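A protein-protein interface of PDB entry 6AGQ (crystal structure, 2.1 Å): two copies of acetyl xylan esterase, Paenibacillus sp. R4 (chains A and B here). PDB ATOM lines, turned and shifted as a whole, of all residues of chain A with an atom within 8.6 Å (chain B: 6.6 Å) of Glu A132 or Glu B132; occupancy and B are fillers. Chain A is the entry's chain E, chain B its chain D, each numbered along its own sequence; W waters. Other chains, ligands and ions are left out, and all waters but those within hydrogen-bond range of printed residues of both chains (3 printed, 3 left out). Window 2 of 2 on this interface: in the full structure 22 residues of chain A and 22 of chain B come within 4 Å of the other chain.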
ATOM      1  N   ASP A  66     -20.182   9.130  -4.604  1.00  0.00           N
ATOM      2  CA  ASP A  66     -19.488   9.918  -3.546  1.00  0.00           C
ATOM      3  C   ASP A  66     -18.393  10.873  -4.085  1.00  0.00           C
ATOM      4  O   ASP A  66     -17.625  11.430  -3.292  1.00  0.00           O
ATOM      5  CB  ASP A  66     -18.883   8.981  -2.480  1.00  0.00           C
ATOM      6  CG  ASP A  66     -17.695   8.095  -3.012  1.00  0.00           C
ATOM      7  OD1 ASP A  66     -17.419   8.029  -4.264  1.00  0.00           O
ATOM      8  OD2 ASP A  66     -17.041   7.440  -2.149  1.00  0.00           O
ATOM      9  N   THR A  68     -15.733   9.948  -6.391  1.00  0.00           N
ATOM     10  CA  THR A  68     -14.543   9.340  -7.001  1.00  0.00           C
ATOM     11  C   THR A  68     -14.588   9.512  -8.535  1.00  0.00           C
ATOM     12  O   THR A  68     -15.613   9.292  -9.120  1.00  0.00           O
ATOM     13  CB  THR A  68     -14.528   7.855  -6.661  1.00  0.00           C
ATOM     14  OG1 THR A  68     -14.606   7.745  -5.233  1.00  0.00           O
ATOM     15  CG2 THR A  68     -13.307   7.182  -7.176  1.00  0.00           C
ATOM     16  N   PRO A  69     -13.490   9.948  -9.167  1.00  0.00           N
ATOM     17  CA  PRO A  69     -13.502   9.969 -10.610  1.00  0.00           C
ATOM     18  C   PRO A  69     -13.200   8.554 -11.127  1.00  0.00           C
ATOM     19  O   PRO A  69     -12.123   8.053 -10.861  1.00  0.00           O
ATOM     20  CB  PRO A  69     -12.363  10.956 -10.984  1.00  0.00           C
ATOM     21  CG  PRO A  69     -11.532  11.071  -9.754  1.00  0.00           C
ATOM     22  CD  PRO A  69     -12.210  10.427  -8.595  1.00  0.00           C
ATOM     23  N   ARG A 121     -12.697   1.166  -8.060  1.00  0.00           N
ATOM     24  CA  ARG A 121     -12.063   2.133  -7.157  1.00  0.00           C
ATOM     25  C   ARG A 121     -11.009   1.591  -6.233  1.00  0.00           C
ATOM     26  O   ARG A 121     -11.173   0.579  -5.515  1.00  0.00           O
ATOM     27  CB  ARG A 121     -13.124   2.901  -6.326  1.00  0.00           C
ATOM     28  CG  ARG A 121     -14.014   2.023  -5.506  1.00  0.00           C
ATOM     29  CD  ARG A 121     -14.916   2.860  -4.675  1.00  0.00           C
ATOM     30  NE  ARG A 121     -15.672   3.855  -5.440  1.00  0.00           N
ATOM     31  CZ  ARG A 121     -16.099   5.014  -4.921  1.00  0.00           C
ATOM     32  NH1 ARG A 121     -16.868   5.845  -5.639  1.00  0.00           N
ATOM     33  NH2 ARG A 121     -15.770   5.352  -3.677  1.00  0.00           N
ATOM     34  N   PRO A 128      -8.828   6.169  -7.846  1.00  0.00           N
ATOM     35  CA  PRO A 128      -8.617   6.086  -6.412  1.00  0.00           C
ATOM     36  C   PRO A 128      -9.920   5.740  -5.732  1.00  0.00           C
ATOM     37  O   PRO A 128     -10.939   5.544  -6.415  1.00  0.00           O
ATOM     38  CB  PRO A 128      -8.166   7.520  -6.072  1.00  0.00           C
ATOM     39  CG  PRO A 128      -9.068   8.335  -6.935  1.00  0.00           C
ATOM     40  CD  PRO A 128      -9.051   7.570  -8.247  1.00  0.00           C
ATOM     41  N   ASP A 129      -9.892   5.691  -4.418  1.00  0.00           N
ATOM     42  CA  ASP A 129     -11.076   5.415  -3.593  1.00  0.00           C
ATOM     43  C   ASP A 129     -11.246   6.591  -2.667  1.00  0.00           C
ATOM     44  O   ASP A 129     -10.438   6.749  -1.800  1.00  0.00           O
ATOM     45  CB  ASP A 129     -10.847   4.150  -2.752  1.00  0.00           C
ATOM     46  CG  ASP A 129     -12.085   3.711  -1.936  1.00  0.00           C
ATOM     47  OD1 ASP A 129     -13.148   4.353  -2.084  1.00  0.00           O
ATOM     48  OD2 ASP A 129     -11.977   2.743  -1.094  1.00  0.00           O
ATOM     49  N   ARG A 130     -12.310   7.383  -2.813  1.00  0.00           N
ATOM     50  CA  ARG A 130     -12.578   8.477  -1.901  1.00  0.00           C
ATOM     51  C   ARG A 130     -13.356   8.113  -0.629  1.00  0.00           C
ATOM     52  O   ARG A 130     -13.454   8.930   0.263  1.00  0.00           O
ATOM     53  CB  ARG A 130     -13.215   9.649  -2.656  1.00  0.00           C
ATOM     54  CG  ARG A 130     -12.316  10.228  -3.752  1.00  0.00           C
ATOM     55  CD  ARG A 130     -11.513  11.423  -3.305  1.00  0.00           C
ATOM     56  NE  ARG A 130     -10.358  11.753  -4.175  1.00  0.00           N
ATOM     57  CZ  ARG A 130      -9.140  11.176  -4.141  1.00  0.00           C
ATOM     58  NH1 ARG A 130      -8.191  11.605  -4.935  1.00  0.00           N
ATOM     59  NH2 ARG A 130      -8.859  10.157  -3.336  1.00  0.00           N
ATOM     60  N   ALA A 131     -13.883   6.893  -0.497  1.00  0.00           N
ATOM     61  CA  ALA A 131     -14.694   6.610   0.699  1.00  0.00           C
ATOM     62  C   ALA A 131     -13.868   6.578   1.982  1.00  0.00           C
ATOM     63  O   ALA A 131     -12.700   6.256   1.956  1.00  0.00           O
ATOM     64  CB  ALA A 131     -15.437   5.288   0.575  1.00  0.00           C
ATOM     65  N   GLU A 132     -14.525   6.853   3.097  1.00  0.00           N
ATOM     66  CA  GLU A 132     -13.918   6.758   4.423  1.00  0.00           C
ATOM     67  C   GLU A 132     -14.519   5.539   5.117  1.00  0.00           C
ATOM     68  O   GLU A 132     -15.706   5.216   4.882  1.00  0.00           O
ATOM     69  CB  GLU A 132     -14.182   8.065   5.202  1.00  0.00           C
ATOM     70  CG  GLU A 132     -13.621   9.332   4.515  1.00  0.00           C
ATOM     71  CD  GLU A 132     -12.080   9.387   4.374  1.00  0.00           C
ATOM     72  OE1 GLU A 132     -11.530  10.520   4.413  1.00  0.00           O
ATOM     73  OE2 GLU A 132     -11.379   8.326   4.235  1.00  0.00           O
ATOM     74  N   TYR A 133     -13.701   4.805   5.876  1.00  0.00           N
ATOM     75  CA  TYR A 133     -14.166   3.595   6.581  1.00  0.00           C
ATOM     76  C   TYR A 133     -13.919   3.827   8.022  1.00  0.00           C
ATOM     77  O   TYR A 133     -13.004   4.532   8.347  1.00  0.00           O
ATOM     78  CB  TYR A 133     -13.360   2.379   6.090  1.00  0.00           C
ATOM     79  CG  TYR A 133     -13.440   2.256   4.629  1.00  0.00           C
ATOM     80  CD1 TYR A 133     -14.580   1.757   4.056  1.00  0.00           C
ATOM     81  CD2 TYR A 133     -12.422   2.726   3.792  1.00  0.00           C
ATOM     82  CE1 TYR A 133     -14.755   1.710   2.689  1.00  0.00           C
ATOM     83  CE2 TYR A 133     -12.554   2.611   2.406  1.00  0.00           C
ATOM     84  CZ  TYR A 133     -13.728   2.111   1.855  1.00  0.00           C
ATOM     85  OH  TYR A 133     -13.973   1.979   0.498  1.00  0.00           O
ATOM     86  N   PRO A 134     -14.704   3.250   8.907  1.00  0.00           N
ATOM     87  CA  PRO A 134     -14.504   3.565  10.335  1.00  0.00           C
ATOM     88  C   PRO A 134     -13.272   2.960  11.028  1.00  0.00           C
ATOM     89  O   PRO A 134     -12.911   3.440  12.103  1.00  0.00           O
ATOM     90  CB  PRO A 134     -15.768   3.006  11.013  1.00  0.00           C
ATOM     91  CG  PRO A 134     -16.361   2.076  10.036  1.00  0.00           C
ATOM     92  CD  PRO A 134     -16.008   2.626   8.673  1.00  0.00           C
ATOM     93  N   GLN A 135     -12.687   1.906  10.457  1.00  0.00           N
ATOM     94  CA  GLN A 135     -11.644   1.141  11.098  1.00  0.00           C
ATOM     95  C   GLN A 135     -10.613   0.887  10.054  1.00  0.00           C
ATOM     96  O   GLN A 135     -10.745   1.337   8.907  1.00  0.00           O
ATOM     97  CB  GLN A 135     -12.178  -0.189  11.660  1.00  0.00           C
ATOM     98  CG  GLN A 135     -13.298  -0.040  12.683  1.00  0.00           C
ATOM     99  CD  GLN A 135     -13.441  -1.255  13.591  1.00  0.00           C
ATOM    100  OE1 GLN A 135     -13.018  -2.364  13.241  1.00  0.00           O
ATOM    101  NE2 GLN A 135     -14.053  -1.059  14.759  1.00  0.00           N
ATOM    102  N   LEU A 144     -12.808  -3.704   4.145  1.00  0.00           N
ATOM    103  CA  LEU A 144     -12.998  -2.290   4.474  1.00  0.00           C
ATOM    104  C   LEU A 144     -14.464  -1.987   4.764  1.00  0.00           C
ATOM    105  O   LEU A 144     -15.343  -2.168   3.907  1.00  0.00           O
ATOM    106  CB  LEU A 144     -12.447  -1.357   3.380  1.00  0.00           C
ATOM    107  CG  LEU A 144     -10.924  -1.373   3.205  1.00  0.00           C
ATOM    108  CD1 LEU A 144     -10.518  -0.614   1.948  1.00  0.00           C
ATOM    109  CD2 LEU A 144     -10.218  -0.781   4.423  1.00  0.00           C
ATOM    110  N   GLY A 145     -14.711  -1.489   5.976  1.00  0.00           N
ATOM    111  CA  GLY A 145     -16.041  -1.217   6.398  1.00  0.00           C
ATOM    112  C   GLY A 145     -16.917  -2.401   6.676  1.00  0.00           C
ATOM    113  O   GLY A 145     -18.159  -2.270   6.667  1.00  0.00           O
ATOM    114  N   ASP A 148     -20.392  -2.670   9.010  1.00  0.00           N
ATOM    115  CA  ASP A 148     -21.564  -1.853   8.721  1.00  0.00           C
ATOM    116  C   ASP A 148     -21.831  -1.787   7.197  1.00  0.00           C
ATOM    117  O   ASP A 148     -20.994  -1.348   6.420  1.00  0.00           O
ATOM    118  CB  ASP A 148     -21.415  -0.433   9.303  1.00  0.00           C
ATOM    119  CG  ASP A 148     -22.763   0.364   9.362  1.00  0.00           C
ATOM    120  OD1 ASP A 148     -23.767   0.011   8.687  1.00  0.00           O
ATOM    121  OD2 ASP A 148     -22.808   1.380  10.107  1.00  0.00           O
ATOM    122  N   ALA A 150     -23.592   0.291   5.426  1.00  0.00           N
ATOM    123  CA  ALA A 150     -23.571   1.634   4.874  1.00  0.00           C
ATOM    124  C   ALA A 150     -22.132   2.084   4.586  1.00  0.00           C
ATOM    125  O   ALA A 150     -21.933   2.972   3.773  1.00  0.00           O
ATOM    126  CB  ALA A 150     -24.278   2.627   5.786  1.00  0.00           C
ATOM    127  N   SER A 151     -21.122   1.469   5.189  1.00  0.00           N
ATOM    128  CA  SER A 151     -19.713   1.899   4.909  1.00  0.00           C
ATOM    129  C   SER A 151     -18.875   0.853   4.155  1.00  0.00           C
ATOM    130  O   SER A 151     -17.712   1.114   3.828  1.00  0.00           O
ATOM    131  CB  SER A 151     -19.002   2.386   6.201  1.00  0.00           C
ATOM    132  OG  SER A 151     -19.071   1.418   7.225  1.00  0.00           O
ATOM    133  N   TYR A 152     -19.488  -0.264   3.797  1.00  0.00           N
ATOM    134  CA  TYR A 152     -18.735  -1.428   3.170  1.00  0.00           C
ATOM    135  C   TYR A 152     -18.197  -1.070   1.814  1.00  0.00           C
ATOM    136  O   TYR A 152     -18.846  -0.359   1.053  1.00  0.00           O
ATOM    137  CB  TYR A 152     -19.564  -2.700   3.166  1.00  0.00           C
ATOM    138  CG  TYR A 152     -18.804  -3.896   2.732  1.00  0.00           C
ATOM    139  CD1 TYR A 152     -17.648  -4.283   3.376  1.00  0.00           C
ATOM    140  CD2 TYR A 152     -19.152  -4.578   1.610  1.00  0.00           C
ATOM    141  CE1 TYR A 152     -16.927  -5.391   2.957  1.00  0.00           C
ATOM    142  CE2 TYR A 152     -18.396  -5.662   1.171  1.00  0.00           C
ATOM    143  CZ  TYR A 152     -17.310  -6.090   1.860  1.00  0.00           C
ATOM    144  OH  TYR A 152     -16.552  -7.170   1.351  1.00  0.00           O
ATOM    145  N   TYR A 153     -16.945  -1.442   1.567  1.00  0.00           N
ATOM    146  CA  TYR A 153     -16.218  -1.137   0.326  1.00  0.00           C
ATOM    147  C   TYR A 153     -17.099  -1.358  -0.919  1.00  0.00           C
ATOM    148  O   TYR A 153     -17.195  -0.473  -1.751  1.00  0.00           O
ATOM    149  CB  TYR A 153     -14.921  -1.991   0.219  1.00  0.00           C
ATOM    150  CG  TYR A 153     -14.201  -1.948  -1.115  1.00  0.00           C
ATOM    151  CD1 TYR A 153     -13.441  -0.836  -1.461  1.00  0.00           C
ATOM    152  CD2 TYR A 153     -14.271  -3.010  -2.010  1.00  0.00           C
ATOM    153  CE1 TYR A 153     -12.799  -0.751  -2.673  1.00  0.00           C
ATOM    154  CE2 TYR A 153     -13.597  -2.943  -3.238  1.00  0.00           C
ATOM    155  CZ  TYR A 153     -12.904  -1.800  -3.580  1.00  0.00           C
ATOM    156  OH  TYR A 153     -12.175  -1.715  -4.752  1.00  0.00           O
ATOM    157  N   GLN A 156     -20.097   1.540  -2.621  1.00  0.00           N
ATOM    158  CA  GLN A 156     -19.810   2.496  -3.709  1.00  0.00           C
ATOM    159  C   GLN A 156     -19.298   1.822  -5.021  1.00  0.00           C
ATOM    160  O   GLN A 156     -19.447   2.402  -6.123  1.00  0.00           O
ATOM    161  CB  GLN A 156     -18.857   3.585  -3.249  1.00  0.00           C
ATOM    162  CG  GLN A 156     -19.500   4.511  -2.213  1.00  0.00           C
ATOM    163  CD  GLN A 156     -20.464   5.510  -2.839  1.00  0.00           C
ATOM    164  OE1 GLN A 156     -20.212   6.015  -3.933  1.00  0.00           O
ATOM    165  NE2 GLN A 156     -21.551   5.813  -2.140  1.00  0.00           N
ATOM    166  N   ASP B  66      -3.767  14.885   9.825  1.00  0.00           N
ATOM    167  CA  ASP B  66      -4.975  15.042   8.973  1.00  0.00           C
ATOM    168  C   ASP B  66      -6.337  14.725   9.651  1.00  0.00           C
ATOM    169  O   ASP B  66      -7.357  14.781   8.993  1.00  0.00           O
ATOM    170  CB  ASP B  66      -4.828  14.192   7.674  1.00  0.00           C
ATOM    171  CG  ASP B  66      -4.751  12.631   7.932  1.00  0.00           C
ATOM    172  OD1 ASP B  66      -4.783  12.146   9.090  1.00  0.00           O
ATOM    173  OD2 ASP B  66      -4.641  11.881   6.945  1.00  0.00           O
ATOM    174  N   PRO B 128      -8.591   3.878  11.326  1.00  0.00           N
ATOM    175  CA  PRO B 128      -8.747   3.933   9.871  1.00  0.00           C
ATOM    176  C   PRO B 128      -7.606   4.801   9.336  1.00  0.00           C
ATOM    177  O   PRO B 128      -6.756   5.230  10.131  1.00  0.00           O
ATOM    178  CB  PRO B 128     -10.109   4.657   9.709  1.00  0.00           C
ATOM    179  CG  PRO B 128     -10.135   5.603  10.871  1.00  0.00           C
ATOM    180  CD  PRO B 128      -9.425   4.902  12.003  1.00  0.00           C
ATOM    181  N   ASP B 129      -7.596   5.007   8.030  1.00  0.00           N
ATOM    182  CA  ASP B 129      -6.675   5.888   7.297  1.00  0.00           C
ATOM    183  C   ASP B 129      -7.486   6.920   6.529  1.00  0.00           C
ATOM    184  O   ASP B 129      -7.986   6.650   5.423  1.00  0.00           O
ATOM    185  CB  ASP B 129      -5.869   5.119   6.257  1.00  0.00           C
ATOM    186  CG  ASP B 129      -4.864   6.044   5.435  1.00  0.00           C
ATOM    187  OD1 ASP B 129      -4.599   7.206   5.859  1.00  0.00           O
ATOM    188  OD2 ASP B 129      -4.350   5.590   4.353  1.00  0.00           O
ATOM    189  N   ARG B 130      -7.542   8.135   7.058  1.00  0.00           N
ATOM    190  CA  ARG B 130      -8.303   9.171   6.410  1.00  0.00           C
ATOM    191  C   ARG B 130      -7.578   9.956   5.288  1.00  0.00           C
ATOM    192  O   ARG B 130      -8.220  10.735   4.630  1.00  0.00           O
ATOM    193  CB  ARG B 130      -8.892  10.109   7.468  1.00  0.00           C
ATOM    194  CG  ARG B 130      -9.827   9.416   8.442  1.00  0.00           C
ATOM    195  CD  ARG B 130     -11.125   9.004   7.738  1.00  0.00           C
ATOM    196  NE  ARG B 130     -11.901   7.898   8.336  1.00  0.00           N
ATOM    197  CZ  ARG B 130     -12.568   7.972   9.484  1.00  0.00           C
ATOM    198  NH1 ARG B 130     -13.256   6.929   9.891  1.00  0.00           N
ATOM    199  NH2 ARG B 130     -12.543   9.076  10.239  1.00  0.00           N
ATOM    200  N   ALA B 131      -6.278   9.765   5.067  1.00  0.00           N
ATOM    201  CA  ALA B 131      -5.611  10.352   3.915  1.00  0.00           C
ATOM    202  C   ALA B 131      -6.306   9.897   2.614  1.00  0.00           C
ATOM    203  O   ALA B 131      -6.882   8.818   2.559  1.00  0.00           O
ATOM    204  CB  ALA B 131      -4.123   9.989   3.867  1.00  0.00           C
ATOM    205  N   GLU B 132      -6.260  10.776   1.608  1.00  0.00           N
ATOM    206  CA  GLU B 132      -6.788  10.541   0.259  1.00  0.00           C
ATOM    207  C   GLU B 132      -5.583  10.439  -0.642  1.00  0.00           C
ATOM    208  O   GLU B 132      -4.617  11.174  -0.460  1.00  0.00           O
ATOM    209  CB  GLU B 132      -7.714  11.702  -0.220  1.00  0.00           C
ATOM    210  CG  GLU B 132      -9.026  11.844   0.563  1.00  0.00           C
ATOM    211  CD  GLU B 132     -10.001  10.682   0.401  1.00  0.00           C
ATOM    212  OE1 GLU B 132     -11.058  10.672   1.095  1.00  0.00           O
ATOM    213  OE2 GLU B 132      -9.752   9.782  -0.437  1.00  0.00           O
ATOM    214  N   TYR B 133      -5.632   9.519  -1.590  1.00  0.00           N
ATOM    215  CA  TYR B 133      -4.514   9.280  -2.493  1.00  0.00           C
ATOM    216  C   TYR B 133      -4.986   9.555  -3.907  1.00  0.00           C
ATOM    217  O   TYR B 133      -6.151   9.354  -4.186  1.00  0.00           O
ATOM    218  CB  TYR B 133      -3.999   7.844  -2.391  1.00  0.00           C
ATOM    219  CG  TYR B 133      -3.649   7.524  -1.005  1.00  0.00           C
ATOM    220  CD1 TYR B 133      -2.431   7.979  -0.459  1.00  0.00           C
ATOM    221  CD2 TYR B 133      -4.529   6.828  -0.186  1.00  0.00           C
ATOM    222  CE1 TYR B 133      -2.097   7.736   0.840  1.00  0.00           C
ATOM    223  CE2 TYR B 133      -4.200   6.591   1.139  1.00  0.00           C
ATOM    224  CZ  TYR B 133      -2.985   7.048   1.632  1.00  0.00           C
ATOM    225  OH  TYR B 133      -2.638   6.854   2.909  1.00  0.00           O
ATOM    226  N   PRO B 134      -4.056   9.960  -4.808  1.00  0.00           N
ATOM    227  CA  PRO B 134      -4.431  10.381  -6.155  1.00  0.00           C
ATOM    228  C   PRO B 134      -4.870   9.244  -7.107  1.00  0.00           C
ATOM    229  O   PRO B 134      -5.500   9.515  -8.099  1.00  0.00           O
ATOM    230  CB  PRO B 134      -3.150  11.047  -6.718  1.00  0.00           C
ATOM    231  CG  PRO B 134      -2.094  10.929  -5.670  1.00  0.00           C
ATOM    232  CD  PRO B 134      -2.605  10.089  -4.549  1.00  0.00           C
ATOM    233  N   SER B 151       2.176  12.923  -0.910  1.00  0.00           N
ATOM    234  CA  SER B 151       0.909  12.153  -0.804  1.00  0.00           C
ATOM    235  C   SER B 151       1.144  10.656  -0.396  1.00  0.00           C
ATOM    236  O   SER B 151       0.171   9.882  -0.227  1.00  0.00           O
ATOM    237  CB  SER B 151       0.199  12.183  -2.183  1.00  0.00           C
ATOM    238  OG  SER B 151       0.986  11.375  -3.125  1.00  0.00           O
HETATM  239  O   HOH W   1     -10.870   5.325   6.090  1.00  0.00           O
HETATM  240  O   HOH W   2      -9.304   2.665   6.796  1.00  0.00           O
HETATM  241  O   HOH W   3      -7.862   7.479  -1.880  1.00  0.00           O
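Among the printed residues, merely in contact across the chains: Pro A128 with Tyr B133, Pro A128 with Pro B134, Glu A132 with Asp B129, Tyr A133 with Pro B128, Pro A134 with Pro B128, Pro A134 with Arg B130 and Gln A135 with Pro B128.
Of the 20 printed residues of chain A, 7 touch a printed residue of chain B. Printed residues of chain A that touch a printed residue of chain B: Pro A128, Asp A129, Arg A130, Glu A132, Tyr A133, Pro A134 and Gln A135. Hydrophobic or aromatic side chains of chain A that line the printed part of chain B: Pro A128. Of the 9 printed residues of chain B, 6 touch a printed residue of chain A. Along chain B the printed residues that touch a printed residue of chain A span positions 128 to 134. Among the printed residues, Asp or Glu carboxylates within 4 Å of a Lys or Arg side-chain nitrogen of the other chain: Arg A130 with Glu B132 (3.1 Å).
Water W3 lies within hydrogen-bond range of the backbone carbonyl oxygen (O) of Asp A129 (2.7 Å), the backbone NH (N) of Tyr B133 (3.0 Å), the guanidinium group (NH2) of Arg A130 (3.2 Å) and the side-chain carboxylate (OE2) of Glu B132 (3.3 Å). Water W2 bridges the backbone carbonyl oxygen of Gln A135 (2.9 Å) and the backbone NH of Asp B129 (3.2 Å). Water W1 bridges N of Tyr A133 and O of Asp B129.
OD1 of Asp B129 is in hydrogen-bond range of N of Ala B131, at 3.2 Å. The side-chain hydroxyl of Tyr B133 sits at hydrogen-bond distance from the side-chain carboxylate of Asp B129, 2.6 Å away. N of Arg A130 lies within hydrogen-bond range of OG1 of Thr A68, at 3.4 Å. The side-chain carboxylate (OD1) of Asp A129 is in salt-bridge range of the guanidinium group (NH2) of Arg A121 (3.2 Å). The backbone NH (N) of Ala A131 lies within hydrogen-bond range of the side-chain carboxylate (OD1) of Asp A129, 3.1 Å away. OD2 of Asp A129 lies within hydrogen-bond range of OH of Tyr A133.
Ala A131 touches none of the printed residues of chain B. Of the printed residues of chain B, Glu A132 touches Asp B129, Arg B130 and Glu B132. Printed residues of chain A within 4 Å of Pro B128: Tyr A133 (3.2 Å), Pro A134 (3.7 Å) and Gln A135 (3.4 Å). Of the printed residues of chain A, Arg B130 touches Glu A132, Tyr A133 and Pro A134. No residue of chain A comes within 4 Å of Ala B131. Of the printed residues of chain A, Glu B132 touches Asp A129, Arg A130 and Glu A132.
O of Tyr A133 lies within hydrogen-bond range of NH1 of Arg B130. The side-chain carboxylate of Glu B132 lies within salt-bridge range of the guanidinium group of Arg A130 (3.1 Å). NH2 of Arg A130 is in hydrogen-bond range of O of Tyr B133, at 2.9 Å. The backbone carbonyl oxygen of Asp A129 lies close to the side-chain carboxylate of Glu B132 (3.4 Å). OE1 of Glu A132 sits close to O of Arg B130, 3.3 Å away. The side-chain carboxylate of Glu B132 sits close to the side-chain carboxylate of Glu A132 (3.4 Å).
Pro A128 touches Tyr B133, and with the chains exchanged Tyr A133 touches Pro B128. Arg A130 touches Glu B132, and with the chains exchanged Glu A132 touches Arg B130. Glu A132 touches its own counterpart, Glu B132. Pro A134 touches Arg B130, but with the chains exchanged Arg A130 does not touch Pro B134 (4.1 Å). Positions printed for both chains: 66, 128, 129, 130, 131, 132, 133, 134 and 151.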
